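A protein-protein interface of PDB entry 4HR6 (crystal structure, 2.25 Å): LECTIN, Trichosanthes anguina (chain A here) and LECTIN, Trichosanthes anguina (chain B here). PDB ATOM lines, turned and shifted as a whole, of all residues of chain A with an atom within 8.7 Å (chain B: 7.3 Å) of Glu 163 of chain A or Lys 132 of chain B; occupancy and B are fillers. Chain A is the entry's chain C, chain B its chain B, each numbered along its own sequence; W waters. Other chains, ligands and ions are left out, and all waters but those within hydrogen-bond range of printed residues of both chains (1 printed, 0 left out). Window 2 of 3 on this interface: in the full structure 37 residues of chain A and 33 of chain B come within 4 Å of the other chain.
Printed residues of chain B within 4 Å of Val 143 of chain A: Gln 125 (3.8 Å) and Tyr 129 (3.2 Å). Of the printed residues of chain B, Asp 147 of chain A touches Gln 125 (2.7 Å), Ala 128 (3.99 Å), Tyr 129 (3.7 Å) and Lys 132 (3.9 Å). Glu 151 of chain A touches none of the printed residues of chain B. Of the printed residues of chain B, Glu 163 of chain A touches Lys 132 (3.2 Å). Val 85 of chain B touches none of the printed residues of chain A. Of the printed residues of chain A, Ala 128 of chain B touches Asp 147. Printed residues of chain A within 4 Å of Tyr 129 of chain B: Val 143 (3.2 Å), Asp 147 (3.7 Å), Cys 149 (3.9 Å) and Cys 164 (3.2 Å). The nearest residue of chain B that does not touch Glu 163 of chain A is Asn 133 of chain B (6.1 Å). The nearest printed residue of chain B that does not touch Asp 146 of chain A is Tyr 129 of chain B (6.5 Å).
The backbone NH of Cys 149 of chain A is in hydrogen-bond range of the backbone carbonyl oxygen of Glu 162 of chain A (2.8 Å). The side-chain amide nitrogen (NE2) of Gln 171 of chain A lies within hydrogen-bond range of the backbone carbonyl oxygen (O) of Glu 163 of chain A, 2.9 Å away. SG of Cys 149 of chain A is disulfide-bonded to SG of Cys 164 of chain A, 2.0 Å away.
Water W1 lies within hydrogen-bond range of OE1 of Gln 125 of chain B and O of Gly 144 of chain A.
Among the printed residues, merely in contact across the chains: Val 143 of chain A with Tyr 129 of chain B (3.2 Å), Glu 163 of chain A with Lys 132 of chain B (3.2 Å), Asp 147 of chain A with Tyr 129 of chain B (3.7 Å), Val 143 of chain A with Gln 125 of chain B (3.8 Å), Cys 149 of chain A with Tyr 129 of chain B (3.9 Å) and Asp 147 of chain A with Ala 128 of chain B (3.99 Å).
NZ of Lys 132 of chain B lies within salt-bridge range of OD1 of Asp 146 of chain A, 3.9 Å away. The side-chain carboxylate (OD1) of Asp 147 of chain A sits at hydrogen-bond distance from the side-chain amide nitrogen (NE2) of Gln 125 of chain B (2.7 Å). OH of Tyr 129 of chain B sits at hydrogen-bond distance from SG of Cys 164 of chain A, at 3.2 Å. The side-chain carboxylate (OD2) of Asp 147 of chain A lies within salt-bridge range of the side-chain amino group (NZ) of Lys 132 of chain B, at 3.9 Å.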
ATOM      1  N   VAL A 143      20.433 -12.569  12.142  1.00  0.00           N
ATOM      2  CA  VAL A 143      21.577 -12.362  13.013  1.00  0.00           C
ATOM      3  C   VAL A 143      21.938 -10.892  13.004  1.00  0.00           C
ATOM      4  O   VAL A 143      22.033 -10.289  11.959  1.00  0.00           O
ATOM      5  CB  VAL A 143      22.785 -13.218  12.562  1.00  0.00           C
ATOM      6  CG1 VAL A 143      23.950 -13.088  13.538  1.00  0.00           C
ATOM      7  CG2 VAL A 143      22.379 -14.680  12.437  1.00  0.00           C
ATOM      8  N   GLY A 144      22.122 -10.318  14.186  1.00  0.00           N
ATOM      9  CA  GLY A 144      22.432  -8.911  14.330  1.00  0.00           C
ATOM     10  C   GLY A 144      23.763  -8.793  15.021  1.00  0.00           C
ATOM     11  O   GLY A 144      24.547  -9.758  15.043  1.00  0.00           O
ATOM     12  N   LEU A 145      24.036  -7.621  15.586  1.00  0.00           N
ATOM     13  CA  LEU A 145      25.367  -7.369  16.104  1.00  0.00           C
ATOM     14  C   LEU A 145      25.711  -8.308  17.254  1.00  0.00           C
ATOM     15  O   LEU A 145      24.831  -8.898  17.898  1.00  0.00           O
ATOM     16  CB  LEU A 145      25.577  -5.905  16.486  1.00  0.00           C
ATOM     17  CG  LEU A 145      25.248  -5.463  17.898  1.00  0.00           C
ATOM     18  CD1 LEU A 145      25.734  -4.031  18.089  1.00  0.00           C
ATOM     19  CD2 LEU A 145      23.753  -5.617  18.145  1.00  0.00           C
ATOM     20  N   ASP A 146      27.015  -8.487  17.443  1.00  0.00           N
ATOM     21  CA  ASP A 146      27.562  -9.394  18.440  1.00  0.00           C
ATOM     22  C   ASP A 146      27.165 -10.821  18.129  1.00  0.00           C
ATOM     23  O   ASP A 146      27.202 -11.687  19.001  1.00  0.00           O
ATOM     24  CB  ASP A 146      27.093  -8.982  19.854  1.00  0.00           C
ATOM     25  CG  ASP A 146      28.177  -9.153  20.912  1.00  0.00           C
ATOM     26  OD1 ASP A 146      29.376  -9.216  20.549  1.00  0.00           O
ATOM     27  OD2 ASP A 146      27.834  -9.208  22.114  1.00  0.00           O
ATOM     28  N   ASP A 147      26.799 -11.074  16.877  1.00  0.00           N
ATOM     29  CA  ASP A 147      26.366 -12.405  16.441  1.00  0.00           C
ATOM     30  C   ASP A 147      25.211 -12.990  17.227  1.00  0.00           C
ATOM     31  O   ASP A 147      25.116 -14.215  17.401  1.00  0.00           O
ATOM     32  CB  ASP A 147      27.547 -13.362  16.463  1.00  0.00           C
ATOM     33  CG  ASP A 147      28.710 -12.813  15.724  1.00  0.00           C
ATOM     34  OD1 ASP A 147      28.568 -12.647  14.495  1.00  0.00           O
ATOM     35  OD2 ASP A 147      29.724 -12.507  16.371  1.00  0.00           O
ATOM     36  N   MET A 148      24.307 -12.121  17.654  1.00  0.00           N
ATOM     37  CA  MET A 148      23.113 -12.565  18.360  1.00  0.00           C
ATOM     38  C   MET A 148      21.924 -12.670  17.415  1.00  0.00           C
ATOM     39  O   MET A 148      21.890 -11.992  16.392  1.00  0.00           O
ATOM     40  CB  MET A 148      22.832 -11.613  19.501  1.00  0.00           C
ATOM     41  CG  MET A 148      23.870 -11.755  20.594  1.00  0.00           C
ATOM     42  SD  MET A 148      23.512 -10.714  22.001  1.00  0.00           S
ATOM     43  CE  MET A 148      22.327 -11.736  22.874  1.00  0.00           C
ATOM     44  N   CYS A 149      20.969 -13.530  17.774  1.00  0.00           N
ATOM     45  CA  CYS A 149      19.829 -13.901  16.935  1.00  0.00           C
ATOM     46  C   CYS A 149      18.514 -13.266  17.422  1.00  0.00           C
ATOM     47  O   CYS A 149      18.244 -13.250  18.629  1.00  0.00           O
ATOM     48  CB  CYS A 149      19.642 -15.418  16.965  1.00  0.00           C
ATOM     49  SG  CYS A 149      20.761 -16.417  15.937  1.00  0.00           S
ATOM     50  N   LEU A 150      17.691 -12.776  16.490  1.00  0.00           N
ATOM     51  CA  LEU A 150      16.331 -12.327  16.807  1.00  0.00           C
ATOM     52  C   LEU A 150      15.506 -13.477  17.337  1.00  0.00           C
ATOM     53  O   LEU A 150      15.406 -14.529  16.707  1.00  0.00           O
ATOM     54  CB  LEU A 150      15.595 -11.780  15.586  1.00  0.00           C
ATOM     55  CG  LEU A 150      15.670 -10.302  15.239  1.00  0.00           C
ATOM     56  CD1 LEU A 150      14.645 -10.060  14.143  1.00  0.00           C
ATOM     57  CD2 LEU A 150      15.395  -9.384  16.415  1.00  0.00           C
ATOM     58  N   GLU A 151      14.898 -13.261  18.503  1.00  0.00           N
ATOM     59  CA  GLU A 151      14.031 -14.261  19.102  1.00  0.00           C
ATOM     60  C   GLU A 151      12.603 -13.724  19.342  1.00  0.00           C
ATOM     61  O   GLU A 151      12.403 -12.563  19.732  1.00  0.00           O
ATOM     62  CB  GLU A 151      14.645 -14.762  20.402  1.00  0.00           C
ATOM     63  CG  GLU A 151      14.030 -16.062  20.886  1.00  0.00           C
ATOM     64  CD  GLU A 151      14.757 -16.623  22.081  1.00  0.00           C
ATOM     65  OE1 GLU A 151      15.918 -17.045  21.921  1.00  0.00           O
ATOM     66  OE2 GLU A 151      14.170 -16.631  23.179  1.00  0.00           O
ATOM     67  N   TRP A 160      13.356  -9.651  20.626  1.00  0.00           N
ATOM     68  CA  TRP A 160      14.652  -9.000  20.823  1.00  0.00           C
ATOM     69  C   TRP A 160      15.795  -9.992  20.550  1.00  0.00           C
ATOM     70  O   TRP A 160      15.570 -11.143  20.162  1.00  0.00           O
ATOM     71  CB  TRP A 160      14.772  -8.411  22.243  1.00  0.00           C
ATOM     72  CG  TRP A 160      14.505  -9.391  23.353  1.00  0.00           C
ATOM     73  CD1 TRP A 160      15.293 -10.435  23.748  1.00  0.00           C
ATOM     74  CD2 TRP A 160      13.362  -9.406  24.215  1.00  0.00           C
ATOM     75  NE1 TRP A 160      14.701 -11.115  24.794  1.00  0.00           N
ATOM     76  CE2 TRP A 160      13.520 -10.491  25.107  1.00  0.00           C
ATOM     77  CE3 TRP A 160      12.220  -8.600  24.325  1.00  0.00           C
ATOM     78  CZ2 TRP A 160      12.575 -10.796  26.087  1.00  0.00           C
ATOM     79  CZ3 TRP A 160      11.285  -8.904  25.298  1.00  0.00           C
ATOM     80  CH2 TRP A 160      11.467  -9.994  26.167  1.00  0.00           C
ATOM     81  N   LEU A 161      17.019  -9.542  20.786  1.00  0.00           N
ATOM     82  CA  LEU A 161      18.204 -10.358  20.552  1.00  0.00           C
ATOM     83  C   LEU A 161      18.591 -11.242  21.733  1.00  0.00           C
ATOM     84  O   LEU A 161      18.726 -10.785  22.870  1.00  0.00           O
ATOM     85  CB  LEU A 161      19.370  -9.458  20.147  1.00  0.00           C
ATOM     86  CG  LEU A 161      19.140  -8.791  18.789  1.00  0.00           C
ATOM     87  CD1 LEU A 161      20.149  -7.677  18.553  1.00  0.00           C
ATOM     88  CD2 LEU A 161      19.192  -9.831  17.690  1.00  0.00           C
ATOM     89  N   GLU A 162      18.742 -12.524  21.439  1.00  0.00           N
ATOM     90  CA  GLU A 162      19.232 -13.503  22.379  1.00  0.00           C
ATOM     91  C   GLU A 162      20.428 -14.194  21.723  1.00  0.00           C
ATOM     92  O   GLU A 162      20.695 -13.990  20.540  1.00  0.00           O
ATOM     93  CB  GLU A 162      18.125 -14.508  22.690  1.00  0.00           C
ATOM     94  CG  GLU A 162      16.988 -13.912  23.521  1.00  0.00           C
ATOM     95  CD  GLU A 162      17.399 -13.602  24.961  1.00  0.00           C
ATOM     96  OE1 GLU A 162      16.930 -12.584  25.519  1.00  0.00           O
ATOM     97  OE2 GLU A 162      18.205 -14.367  25.534  1.00  0.00           O
ATOM     98  N   GLU A 163      21.151 -14.985  22.505  1.00  0.00           N
ATOM     99  CA  GLU A 163      22.239 -15.785  21.996  1.00  0.00           C
ATOM    100  C   GLU A 163      21.651 -16.839  21.074  1.00  0.00           C
ATOM    101  O   GLU A 163      20.672 -17.502  21.427  1.00  0.00           O
ATOM    102  CB  GLU A 163      22.994 -16.470  23.143  1.00  0.00           C
ATOM    103  CG  GLU A 163      24.470 -16.711  22.868  1.00  0.00           C
ATOM    104  CD  GLU A 163      25.316 -15.450  23.000  1.00  0.00           C
ATOM    105  OE1 GLU A 163      26.130 -15.178  22.091  1.00  0.00           O
ATOM    106  OE2 GLU A 163      25.170 -14.727  24.010  1.00  0.00           O
ATOM    107  N   CYS A 164      22.263 -17.009  19.907  1.00  0.00           N
ATOM    108  CA  CYS A 164      21.813 -18.005  18.947  1.00  0.00           C
ATOM    109  C   CYS A 164      21.944 -19.401  19.496  1.00  0.00           C
ATOM    110  O   CYS A 164      22.953 -19.729  20.111  1.00  0.00           O
ATOM    111  CB  CYS A 164      22.628 -17.919  17.653  1.00  0.00           C
ATOM    112  SG  CYS A 164      22.536 -16.308  16.879  1.00  0.00           S
ATOM    113  N   VAL A 165      20.929 -20.223  19.246  1.00  0.00           N
ATOM    114  CA  VAL A 165      20.934 -21.618  19.659  1.00  0.00           C
ATOM    115  C   VAL A 165      20.363 -22.435  18.502  1.00  0.00           C
ATOM    116  O   VAL A 165      19.173 -22.328  18.198  1.00  0.00           O
ATOM    117  CB  VAL A 165      20.084 -21.855  20.927  1.00  0.00           C
ATOM    118  CG1 VAL A 165      20.288 -23.278  21.436  1.00  0.00           C
ATOM    119  CG2 VAL A 165      20.419 -20.837  22.010  1.00  0.00           C
ATOM    120  N   PRO A 166      21.207 -23.243  17.841  1.00  0.00           N
ATOM    121  CA  PRO A 166      20.723 -23.934  16.643  1.00  0.00           C
ATOM    122  C   PRO A 166      19.474 -24.759  16.926  1.00  0.00           C
ATOM    123  O   PRO A 166      19.369 -25.377  17.986  1.00  0.00           O
ATOM    124  CB  PRO A 166      21.899 -24.844  16.245  1.00  0.00           C
ATOM    125  CG  PRO A 166      22.792 -24.901  17.438  1.00  0.00           C
ATOM    126  CD  PRO A 166      22.599 -23.604  18.165  1.00  0.00           C
ATOM    127  N   LYS A 168      16.577 -23.791  17.772  1.00  0.00           N
ATOM    128  CA  LYS A 168      15.622 -23.189  18.700  1.00  0.00           C
ATOM    129  C   LYS A 168      14.472 -22.582  17.888  1.00  0.00           C
ATOM    130  O   LYS A 168      14.687 -21.723  17.023  1.00  0.00           O
ATOM    131  CB  LYS A 168      16.265 -22.126  19.590  1.00  0.00           C
ATOM    132  CG  LYS A 168      15.355 -21.725  20.741  1.00  0.00           C
ATOM    133  CD  LYS A 168      15.947 -20.639  21.614  1.00  0.00           C
ATOM    134  CE  LYS A 168      15.022 -20.318  22.780  1.00  0.00           C
ATOM    135  NZ  LYS A 168      15.748 -19.567  23.841  1.00  0.00           N
ATOM    136  N   GLN A 171      13.674 -18.817  17.319  1.00  0.00           N
ATOM    137  CA  GLN A 171      14.678 -18.078  16.552  1.00  0.00           C
ATOM    138  C   GLN A 171      14.541 -18.292  15.038  1.00  0.00           C
ATOM    139  O   GLN A 171      15.368 -17.804  14.268  1.00  0.00           O
ATOM    140  CB  GLN A 171      16.086 -18.461  17.040  1.00  0.00           C
ATOM    141  CG  GLN A 171      16.343 -18.010  18.477  1.00  0.00           C
ATOM    142  CD  GLN A 171      17.799 -18.087  18.898  1.00  0.00           C
ATOM    143  OE1 GLN A 171      18.600 -18.787  18.280  1.00  0.00           O
ATOM    144  NE2 GLN A 171      18.149 -17.367  19.971  1.00  0.00           N
ATOM    145  N   VAL A 242      22.264  -4.497  23.295  1.00  0.00           N
ATOM    146  CA  VAL A 242      21.474  -5.725  23.336  1.00  0.00           C
ATOM    147  C   VAL A 242      20.587  -5.834  24.594  1.00  0.00           C
ATOM    148  O   VAL A 242      19.451  -6.320  24.523  1.00  0.00           O
ATOM    149  CB  VAL A 242      22.388  -6.974  23.222  1.00  0.00           C
ATOM    150  CG1 VAL A 242      23.643  -6.842  24.086  1.00  0.00           C
ATOM    151  CG2 VAL A 242      21.627  -8.244  23.583  1.00  0.00           C
ATOM    152  N   LYS A 245      16.743  -4.809  25.311  1.00  0.00           N
ATOM    153  CA  LYS A 245      15.643  -5.617  24.781  1.00  0.00           C
ATOM    154  C   LYS A 245      14.706  -4.862  23.813  1.00  0.00           C
ATOM    155  O   LYS A 245      13.555  -5.263  23.643  1.00  0.00           O
ATOM    156  CB  LYS A 245      14.837  -6.233  25.934  1.00  0.00           C
ATOM    157  CG  LYS A 245      15.236  -7.653  26.279  1.00  0.00           C
ATOM    158  CD  LYS A 245      16.594  -7.727  26.941  1.00  0.00           C
ATOM    159  CE  LYS A 245      16.924  -9.158  27.345  1.00  0.00           C
ATOM    160  NZ  LYS A 245      15.924  -9.721  28.301  1.00  0.00           N
ATOM    161  N   VAL B  85      39.298 -20.955  13.627  1.00  0.00           N
ATOM    162  CA  VAL B  85      40.432 -20.191  14.103  1.00  0.00           C
ATOM    163  C   VAL B  85      41.717 -21.016  14.071  1.00  0.00           C
ATOM    164  O   VAL B  85      42.743 -20.552  13.575  1.00  0.00           O
ATOM    165  CB  VAL B  85      40.183 -19.689  15.529  1.00  0.00           C
ATOM    166  CG1 VAL B  85      41.400 -18.935  16.047  1.00  0.00           C
ATOM    167  CG2 VAL B  85      38.939 -18.805  15.555  1.00  0.00           C
ATOM    168  N   GLN B 125      29.521 -14.805   7.977  1.00  0.00           N
ATOM    169  CA  GLN B 125      28.810 -15.066   9.224  1.00  0.00           C
ATOM    170  C   GLN B 125      29.092 -16.466   9.744  1.00  0.00           C
ATOM    171  O   GLN B 125      29.284 -16.647  10.932  1.00  0.00           O
ATOM    172  CB  GLN B 125      27.293 -14.833   9.088  1.00  0.00           C
ATOM    173  CG  GLN B 125      26.537 -14.866  10.426  1.00  0.00           C
ATOM    174  CD  GLN B 125      27.048 -13.831  11.418  1.00  0.00           C
ATOM    175  OE1 GLN B 125      27.044 -12.649  11.136  1.00  0.00           O
ATOM    176  NE2 GLN B 125      27.517 -14.281  12.570  1.00  0.00           N
ATOM    177  N   VAL B 127      31.857 -18.092   9.316  1.00  0.00           N
ATOM    178  CA  VAL B 127      33.203 -18.039   9.869  1.00  0.00           C
ATOM    179  C   VAL B 127      33.242 -17.283  11.202  1.00  0.00           C
ATOM    180  O   VAL B 127      33.898 -17.741  12.143  1.00  0.00           O
ATOM    181  CB  VAL B 127      34.225 -17.476   8.868  1.00  0.00           C
ATOM    182  CG1 VAL B 127      35.595 -17.289   9.520  1.00  0.00           C
ATOM    183  CG2 VAL B 127      34.333 -18.399   7.657  1.00  0.00           C
ATOM    184  N   ALA B 128      32.542 -16.149  11.288  1.00  0.00           N
ATOM    185  CA  ALA B 128      32.494 -15.367  12.523  1.00  0.00           C
ATOM    186  C   ALA B 128      32.053 -16.213  13.723  1.00  0.00           C
ATOM    187  O   ALA B 128      32.638 -16.119  14.786  1.00  0.00           O
ATOM    188  CB  ALA B 128      31.589 -14.163  12.369  1.00  0.00           C
ATOM    189  N   TYR B 129      31.050 -17.062  13.538  1.00  0.00           N
ATOM    190  CA  TYR B 129      30.623 -17.969  14.593  1.00  0.00           C
ATOM    191  C   TYR B 129      31.739 -18.871  15.106  1.00  0.00           C
ATOM    192  O   TYR B 129      31.749 -19.196  16.303  1.00  0.00           O
ATOM    193  CB  TYR B 129      29.479 -18.866  14.131  1.00  0.00           C
ATOM    194  CG  TYR B 129      28.095 -18.237  14.167  1.00  0.00           C
ATOM    195  CD1 TYR B 129      27.653 -17.491  15.270  1.00  0.00           C
ATOM    196  CD2 TYR B 129      27.204 -18.439  13.113  1.00  0.00           C
ATOM    197  CE1 TYR B 129      26.374 -16.941  15.295  1.00  0.00           C
ATOM    198  CE2 TYR B 129      25.930 -17.901  13.131  1.00  0.00           C
ATOM    199  CZ  TYR B 129      25.517 -17.149  14.218  1.00  0.00           C
ATOM    200  OH  TYR B 129      24.239 -16.624  14.199  1.00  0.00           O
ATOM    201  N   SER B 130      32.640 -19.303  14.206  1.00  0.00           N
ATOM    202  CA  SER B 130      33.726 -20.219  14.567  1.00  0.00           C
ATOM    203  C   SER B 130      34.702 -19.490  15.467  1.00  0.00           C
ATOM    204  O   SER B 130      35.311 -20.107  16.319  1.00  0.00           O
ATOM    205  CB  SER B 130      34.469 -20.783  13.327  1.00  0.00           C
ATOM    206  OG  SER B 130      35.384 -19.825  12.770  1.00  0.00           O
ATOM    207  N   PHE B 131      34.874 -18.188  15.245  1.00  0.00           N
ATOM    208  CA  PHE B 131      35.671 -17.351  16.133  1.00  0.00           C
ATOM    209  C   PHE B 131      34.995 -17.167  17.495  1.00  0.00           C
ATOM    210  O   PHE B 131      35.683 -17.157  18.515  1.00  0.00           O
ATOM    211  CB  PHE B 131      35.918 -15.961  15.529  1.00  0.00           C
ATOM    212  CG  PHE B 131      37.082 -15.891  14.569  1.00  0.00           C
ATOM    213  CD1 PHE B 131      38.294 -15.353  14.968  1.00  0.00           C
ATOM    214  CD2 PHE B 131      36.962 -16.347  13.262  1.00  0.00           C
ATOM    215  CE1 PHE B 131      39.360 -15.263  14.085  1.00  0.00           C
ATOM    216  CE2 PHE B 131      38.029 -16.268  12.386  1.00  0.00           C
ATOM    217  CZ  PHE B 131      39.230 -15.727  12.794  1.00  0.00           C
ATOM    218  N   LYS B 132      33.665 -17.023  17.511  1.00  0.00           N
ATOM    219  CA  LYS B 132      32.928 -16.773  18.762  1.00  0.00           C
ATOM    220  C   LYS B 132      32.935 -17.988  19.687  1.00  0.00           C
ATOM    221  O   LYS B 132      33.394 -17.903  20.820  1.00  0.00           O
ATOM    222  CB  LYS B 132      31.484 -16.353  18.489  1.00  0.00           C
ATOM    223  CG  LYS B 132      30.826 -15.686  19.686  1.00  0.00           C
ATOM    224  CD  LYS B 132      29.334 -15.487  19.480  1.00  0.00           C
ATOM    225  CE  LYS B 132      28.776 -14.422  20.420  1.00  0.00           C
ATOM    226  NZ  LYS B 132      29.411 -13.085  20.197  1.00  0.00           N
ATOM    227  N   ASN B 133      32.458 -19.120  19.181  1.00  0.00           N
ATOM    228  CA  ASN B 133      32.381 -20.361  19.952  1.00  0.00           C
ATOM    229  C   ASN B 133      33.687 -21.158  19.979  1.00  0.00           C
ATOM    230  O   ASN B 133      33.728 -22.256  20.532  1.00  0.00           O
ATOM    231  CB  ASN B 133      31.295 -21.258  19.369  1.00  0.00           C
ATOM    232  CG  ASN B 133      29.988 -20.529  19.156  1.00  0.00           C
ATOM    233  OD1 ASN B 133      29.667 -19.569  19.864  1.00  0.00           O
ATOM    234  ND2 ASN B 133      29.223 -20.979  18.172  1.00  0.00           N
ATOM    235  N   GLU B 134      34.744 -20.622  19.370  1.00  0.00           N
ATOM    236  CA  GLU B 134      36.027 -21.318  19.268  1.00  0.00           C
ATOM    237  C   GLU B 134      35.833 -22.802  18.938  1.00  0.00           C
ATOM    238  O   GLU B 134      36.436 -23.695  19.540  1.00  0.00           O
ATOM    239  CB  GLU B 134      36.857 -21.088  20.540  1.00  0.00           C
ATOM    240  CG  GLU B 134      37.447 -19.678  20.601  1.00  0.00           C
ATOM    241  CD  GLU B 134      38.742 -19.596  21.389  1.00  0.00           C
ATOM    242  OE1 GLU B 134      38.673 -19.726  22.627  1.00  0.00           O
ATOM    243  OE2 GLU B 134      39.822 -19.392  20.775  1.00  0.00           O
ATOM    244  N   LYS B 135      34.960 -23.032  17.966  1.00  0.00           N
ATOM    245  CA  LYS B 135      34.638 -24.352  17.487  1.00  0.00           C
ATOM    246  C   LYS B 135      34.719 -24.395  15.960  1.00  0.00           C
ATOM    247  O   LYS B 135      34.310 -23.474  15.259  1.00  0.00           O
ATOM    248  CB  LYS B 135      33.227 -24.756  17.926  1.00  0.00           C
ATOM    249  CG  LYS B 135      33.131 -25.314  19.339  1.00  0.00           C
ATOM    250  CD  LYS B 135      33.541 -26.782  19.390  1.00  0.00           C
ATOM    251  CE  LYS B 135      33.009 -27.470  20.641  1.00  0.00           C
ATOM    252  NZ  LYS B 135      33.595 -26.914  21.892  1.00  0.00           N
HETATM  253  O   HOH W   1      26.461 -10.206  12.746  1.00  0.00           O
